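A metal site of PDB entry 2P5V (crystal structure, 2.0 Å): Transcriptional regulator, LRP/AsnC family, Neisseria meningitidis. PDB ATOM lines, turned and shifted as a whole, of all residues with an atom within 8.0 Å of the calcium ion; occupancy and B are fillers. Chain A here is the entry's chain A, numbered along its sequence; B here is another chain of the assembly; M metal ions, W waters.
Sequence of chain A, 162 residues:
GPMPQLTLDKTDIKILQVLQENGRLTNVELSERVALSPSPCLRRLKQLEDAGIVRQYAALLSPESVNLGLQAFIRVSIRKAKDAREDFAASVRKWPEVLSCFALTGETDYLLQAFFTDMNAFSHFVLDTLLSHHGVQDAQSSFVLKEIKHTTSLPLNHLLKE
Water W1 lies within hydrogen-bond range of N of Asp 109 and OG of Ser 77 of chain A.
N of Ser 77 of chain B sits at hydrogen-bond distance from O of Asp 138 of chain B, 2.8 Å away.
The side-chain hydroxyl of Ser 77 of chain A is in hydrogen-bond range of the side-chain carboxylate of Asp 109, at 3.4 Å.
The backbone NH of Asp 109 sits close to the backbone carbonyl oxygen of Val 76.
OD2 of Asp 109 sits at hydrogen-bond distance from N of Ile 78 (3.0 Å).
O of Asp 109 sits at hydrogen-bond distance from N of Leu 104 (3.1 Å).
The backbone carbonyl oxygen (O) of Glu 107 binds the calcium ion (2.3 Å).
OD1 of Asp 109 binds the calcium ion.
The calcium ion is bound by OD2 of Asp 138 of chain B, at 2.6 Å.
Slightly farther from the calcium ion lies the side-chain carboxylate (OD1) of Asp 138 of chain B (3.1 Å).
Three residues have an atom within 4 Å of the calcium ion: Glu 107, Asp 109 and Asp 138 of chain B.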
ATOM      1  N   VAL A  76     -17.689 -18.938  -8.712  1.00  0.00           N
ATOM      2  CA  VAL A  76     -17.917 -19.453 -10.068  1.00  0.00           C
ATOM      3  C   VAL A  76     -16.820 -20.396 -10.531  1.00  0.00           C
ATOM      4  O   VAL A  76     -15.644 -20.080 -10.414  1.00  0.00           O
ATOM      5  CB  VAL A  76     -17.986 -18.306 -11.110  1.00  0.00           C
ATOM      6  CG1 VAL A  76     -18.107 -18.866 -12.536  1.00  0.00           C
ATOM      7  CG2 VAL A  76     -19.168 -17.413 -10.802  1.00  0.00           C
ATOM      8  N   SER A  77     -17.236 -21.539 -11.077  1.00  0.00           N
ATOM      9  CA  SER A  77     -16.338 -22.463 -11.745  1.00  0.00           C
ATOM     10  C   SER A  77     -16.440 -22.261 -13.249  1.00  0.00           C
ATOM     11  O   SER A  77     -17.517 -22.347 -13.830  1.00  0.00           O
ATOM     12  CB  SER A  77     -16.669 -23.908 -11.374  1.00  0.00           C
ATOM     13  OG  SER A  77     -15.639 -24.760 -11.807  1.00  0.00           O
ATOM     14  N   ILE A  78     -15.303 -22.015 -13.874  1.00  0.00           N
ATOM     15  CA  ILE A  78     -15.221 -21.744 -15.299  1.00  0.00           C
ATOM     16  C   ILE A  78     -15.075 -23.068 -16.053  1.00  0.00           C
ATOM     17  O   ILE A  78     -14.517 -24.028 -15.526  1.00  0.00           O
ATOM     18  CB  ILE A  78     -14.010 -20.801 -15.568  1.00  0.00           C
ATOM     19  CG1 ILE A  78     -14.216 -19.995 -16.855  1.00  0.00           C
ATOM     20  CG2 ILE A  78     -12.704 -21.575 -15.545  1.00  0.00           C
ATOM     21  CD1 ILE A  78     -15.149 -18.803 -16.638  1.00  0.00           C
ATOM     22  N   ARG A  85     -12.462 -18.148 -20.030  1.00  0.00           N
ATOM     23  CA  ARG A  85     -12.060 -17.115 -19.075  1.00  0.00           C
ATOM     24  C   ARG A  85     -12.138 -15.708 -19.666  1.00  0.00           C
ATOM     25  O   ARG A  85     -12.588 -14.779 -19.004  1.00  0.00           O
ATOM     26  CB  ARG A  85     -10.630 -17.340 -18.602  1.00  0.00           C
ATOM     27  CG  ARG A  85     -10.461 -18.617 -17.805  1.00  0.00           C
ATOM     28  CD  ARG A  85      -9.089 -18.719 -17.168  1.00  0.00           C
ATOM     29  NE  ARG A  85      -9.108 -19.717 -16.104  1.00  0.00           N
ATOM     30  CZ  ARG A  85      -9.047 -19.470 -14.802  1.00  0.00           C
ATOM     31  NH1 ARG A  85      -8.940 -18.232 -14.329  1.00  0.00           N
ATOM     32  NH2 ARG A  85      -9.083 -20.490 -13.948  1.00  0.00           N
ATOM     33  N   LEU A 104      -9.054 -16.408  -8.160  1.00  0.00           N
ATOM     34  CA  LEU A 104      -8.457 -16.729  -6.852  1.00  0.00           C
ATOM     35  C   LEU A 104      -7.656 -18.024  -6.877  1.00  0.00           C
ATOM     36  O   LEU A 104      -7.807 -18.810  -7.784  1.00  0.00           O
ATOM     37  CB  LEU A 104      -9.552 -16.875  -5.782  1.00  0.00           C
ATOM     38  CG  LEU A 104     -10.412 -15.660  -5.405  1.00  0.00           C
ATOM     39  CD1 LEU A 104     -11.323 -16.050  -4.268  1.00  0.00           C
ATOM     40  CD2 LEU A 104      -9.546 -14.482  -5.013  1.00  0.00           C
ATOM     41  N   THR A 105      -6.849 -18.242  -5.833  1.00  0.00           N
ATOM     42  CA  THR A 105      -5.897 -19.366  -5.749  1.00  0.00           C
ATOM     43  C   THR A 105      -6.421 -20.715  -5.238  1.00  0.00           C
ATOM     44  O   THR A 105      -5.735 -21.731  -5.378  1.00  0.00           O
ATOM     45  CB  THR A 105      -4.756 -19.034  -4.774  1.00  0.00           C
ATOM     46  OG1 THR A 105      -5.316 -18.641  -3.515  1.00  0.00           O
ATOM     47  CG2 THR A 105      -3.853 -17.919  -5.350  1.00  0.00           C
ATOM     48  N   GLY A 106      -7.604 -20.739  -4.635  1.00  0.00           N
ATOM     49  CA  GLY A 106      -8.125 -21.980  -4.088  1.00  0.00           C
ATOM     50  C   GLY A 106      -9.029 -22.703  -5.048  1.00  0.00           C
ATOM     51  O   GLY A 106      -8.819 -22.695  -6.256  1.00  0.00           O
ATOM     52  N   GLU A 107     -10.047 -23.365  -4.495  1.00  0.00           N
ATOM     53  CA  GLU A 107     -10.945 -24.202  -5.295  1.00  0.00           C
ATOM     54  C   GLU A 107     -11.938 -23.381  -6.107  1.00  0.00           C
ATOM     55  O   GLU A 107     -12.428 -23.843  -7.123  1.00  0.00           O
ATOM     56  CB  GLU A 107     -11.691 -25.209  -4.410  1.00  0.00           C
ATOM     57  CG  GLU A 107     -12.589 -24.595  -3.337  1.00  0.00           C
ATOM     58  CD  GLU A 107     -13.289 -25.649  -2.488  1.00  0.00           C
ATOM     59  OE1 GLU A 107     -12.964 -26.860  -2.612  1.00  0.00           O
ATOM     60  OE2 GLU A 107     -14.171 -25.259  -1.682  1.00  0.00           O
ATOM     61  N   THR A 108     -12.238 -22.173  -5.654  1.00  0.00           N
ATOM     62  CA  THR A 108     -13.107 -21.272  -6.399  1.00  0.00           C
ATOM     63  C   THR A 108     -12.285 -20.547  -7.454  1.00  0.00           C
ATOM     64  O   THR A 108     -11.325 -19.852  -7.106  1.00  0.00           O
ATOM     65  CB  THR A 108     -13.766 -20.247  -5.459  1.00  0.00           C
ATOM     66  OG1 THR A 108     -14.522 -20.943  -4.458  1.00  0.00           O
ATOM     67  CG2 THR A 108     -14.654 -19.282  -6.235  1.00  0.00           C
ATOM     68  N   ASP A 109     -12.670 -20.706  -8.712  1.00  0.00           N
ATOM     69  CA  ASP A 109     -11.962 -20.083  -9.831  1.00  0.00           C
ATOM     70  C   ASP A 109     -12.118 -18.561  -9.832  1.00  0.00           C
ATOM     71  O   ASP A 109     -11.133 -17.832  -9.976  1.00  0.00           O
ATOM     72  CB  ASP A 109     -12.488 -20.619 -11.162  1.00  0.00           C
ATOM     73  CG  ASP A 109     -12.331 -22.131 -11.286  1.00  0.00           C
ATOM     74  OD1 ASP A 109     -11.613 -22.719 -10.446  1.00  0.00           O
ATOM     75  OD2 ASP A 109     -12.913 -22.711 -12.213  1.00  0.00           O
ATOM     76  N   TYR A 110     -13.352 -18.105  -9.706  1.00  0.00           N
ATOM     77  CA  TYR A 110     -13.658 -16.677  -9.631  1.00  0.00           C
ATOM     78  C   TYR A 110     -14.633 -16.397  -8.519  1.00  0.00           C
ATOM     79  O   TYR A 110     -15.638 -17.090  -8.375  1.00  0.00           O
ATOM     80  CB  TYR A 110     -14.299 -16.183 -10.922  1.00  0.00           C
ATOM     81  CG  TYR A 110     -13.411 -16.248 -12.122  1.00  0.00           C
ATOM     82  CD1 TYR A 110     -12.626 -15.159 -12.490  1.00  0.00           C
ATOM     83  CD2 TYR A 110     -13.367 -17.389 -12.918  1.00  0.00           C
ATOM     84  CE1 TYR A 110     -11.810 -15.202 -13.611  1.00  0.00           C
ATOM     85  CE2 TYR A 110     -12.559 -17.453 -14.028  1.00  0.00           C
ATOM     86  CZ  TYR A 110     -11.789 -16.355 -14.382  1.00  0.00           C
ATOM     87  OH  TYR A 110     -10.987 -16.418 -15.504  1.00  0.00           O
ATOM     88  N   GLN A 137     -19.200 -23.126 -15.890  1.00  0.00           N
ATOM     89  CA  GLN A 137     -19.463 -24.529 -15.573  1.00  0.00           C
ATOM     90  C   GLN A 137     -20.457 -24.607 -14.410  1.00  0.00           C
ATOM     91  O   GLN A 137     -21.437 -25.324 -14.477  1.00  0.00           O
ATOM     92  CB  GLN A 137     -18.154 -25.219 -15.211  1.00  0.00           C
ATOM     93  CG  GLN A 137     -18.219 -26.716 -14.973  1.00  0.00           C
ATOM     94  CD  GLN A 137     -16.895 -27.266 -14.457  1.00  0.00           C
ATOM     95  OE1 GLN A 137     -15.860 -27.163 -15.135  1.00  0.00           O
ATOM     96  NE2 GLN A 137     -16.909 -27.819 -13.245  1.00  0.00           N
ATOM     97  N   SER B  77      -5.781 -31.534 -10.409  1.00  0.00           N
ATOM     98  CA  SER B  77      -6.710 -32.533 -10.875  1.00  0.00           C
ATOM     99  C   SER B  77      -6.417 -32.697 -12.335  1.00  0.00           C
ATOM    100  O   SER B  77      -6.426 -31.741 -13.107  1.00  0.00           O
ATOM    101  CB  SER B  77      -8.169 -32.095 -10.687  1.00  0.00           C
ATOM    102  OG  SER B  77      -8.432 -31.746  -9.343  1.00  0.00           O
ATOM    103  N   LEU B 131      -2.640 -23.975 -15.801  1.00  0.00           N
ATOM    104  CA  LEU B 131      -4.060 -24.161 -16.097  1.00  0.00           C
ATOM    105  C   LEU B 131      -4.310 -24.275 -17.578  1.00  0.00           C
ATOM    106  O   LEU B 131      -5.293 -24.886 -17.994  1.00  0.00           O
ATOM    107  CB  LEU B 131      -4.896 -23.018 -15.504  1.00  0.00           C
ATOM    108  CG  LEU B 131      -4.916 -22.990 -13.971  1.00  0.00           C
ATOM    109  CD1 LEU B 131      -5.640 -21.764 -13.438  1.00  0.00           C
ATOM    110  CD2 LEU B 131      -5.550 -24.259 -13.428  1.00  0.00           C
ATOM    111  N   GLN B 137      -7.196 -30.304 -15.512  1.00  0.00           N
ATOM    112  CA  GLN B 137      -8.606 -29.990 -15.337  1.00  0.00           C
ATOM    113  C   GLN B 137      -8.777 -28.833 -14.360  1.00  0.00           C
ATOM    114  O   GLN B 137      -9.583 -27.944 -14.591  1.00  0.00           O
ATOM    115  CB  GLN B 137      -9.320 -31.218 -14.782  1.00  0.00           C
ATOM    116  CG  GLN B 137     -10.818 -31.096 -14.596  1.00  0.00           C
ATOM    117  CD  GLN B 137     -11.340 -32.217 -13.703  1.00  0.00           C
ATOM    118  OE1 GLN B 137     -11.589 -33.333 -14.176  1.00  0.00           O
ATOM    119  NE2 GLN B 137     -11.475 -31.929 -12.407  1.00  0.00           N
ATOM    120  N   ASP B 138      -8.035 -28.880 -13.249  1.00  0.00           N
ATOM    121  CA  ASP B 138      -8.099 -27.821 -12.234  1.00  0.00           C
ATOM    122  C   ASP B 138      -6.903 -27.870 -11.287  1.00  0.00           C
ATOM    123  O   ASP B 138      -6.207 -28.885 -11.207  1.00  0.00           O
ATOM    124  CB  ASP B 138      -9.406 -27.921 -11.427  1.00  0.00           C
ATOM    125  CG  ASP B 138     -10.031 -26.542 -11.171  1.00  0.00           C
ATOM    126  OD1 ASP B 138      -9.291 -25.545 -11.054  1.00  0.00           O
ATOM    127  OD2 ASP B 138     -11.286 -26.470 -11.094  1.00  0.00           O
ATOM    128  N   ALA B 139      -6.681 -26.764 -10.577  1.00  0.00           N
ATOM    129  CA  ALA B 139      -5.633 -26.652  -9.574  1.00  0.00           C
ATOM    130  C   ALA B 139      -6.092 -25.759  -8.427  1.00  0.00           C
ATOM    131  O   ALA B 139      -6.880 -24.856  -8.620  1.00  0.00           O
ATOM    132  CB  ALA B 139      -4.347 -26.117 -10.190  1.00  0.00           C
ATOM    133  N   GLN B 140      -5.617 -26.055  -7.227  1.00  0.00           N
ATOM    134  CA  GLN B 140      -5.878 -25.204  -6.075  1.00  0.00           C
ATOM    135  C   GLN B 140      -4.689 -25.310  -5.155  1.00  0.00           C
ATOM    136  O   GLN B 140      -4.106 -26.372  -5.024  1.00  0.00           O
ATOM    137  CB  GLN B 140      -7.164 -25.614  -5.359  1.00  0.00           C
ATOM    138  CG  GLN B 140      -7.177 -27.039  -4.843  1.00  0.00           C
ATOM    139  CD  GLN B 140      -8.454 -27.349  -4.102  1.00  0.00           C
ATOM    140  OE1 GLN B 140      -9.454 -27.739  -4.698  1.00  0.00           O
ATOM    141  NE2 GLN B 140      -8.416 -27.171  -2.789  1.00  0.00           N
HETATM  142 CA    CA M   1     -11.610 -24.792  -9.079  1.00  0.00          CA
HETATM  143  O   HOH W   1     -14.516 -23.190  -9.158  1.00  0.00           O
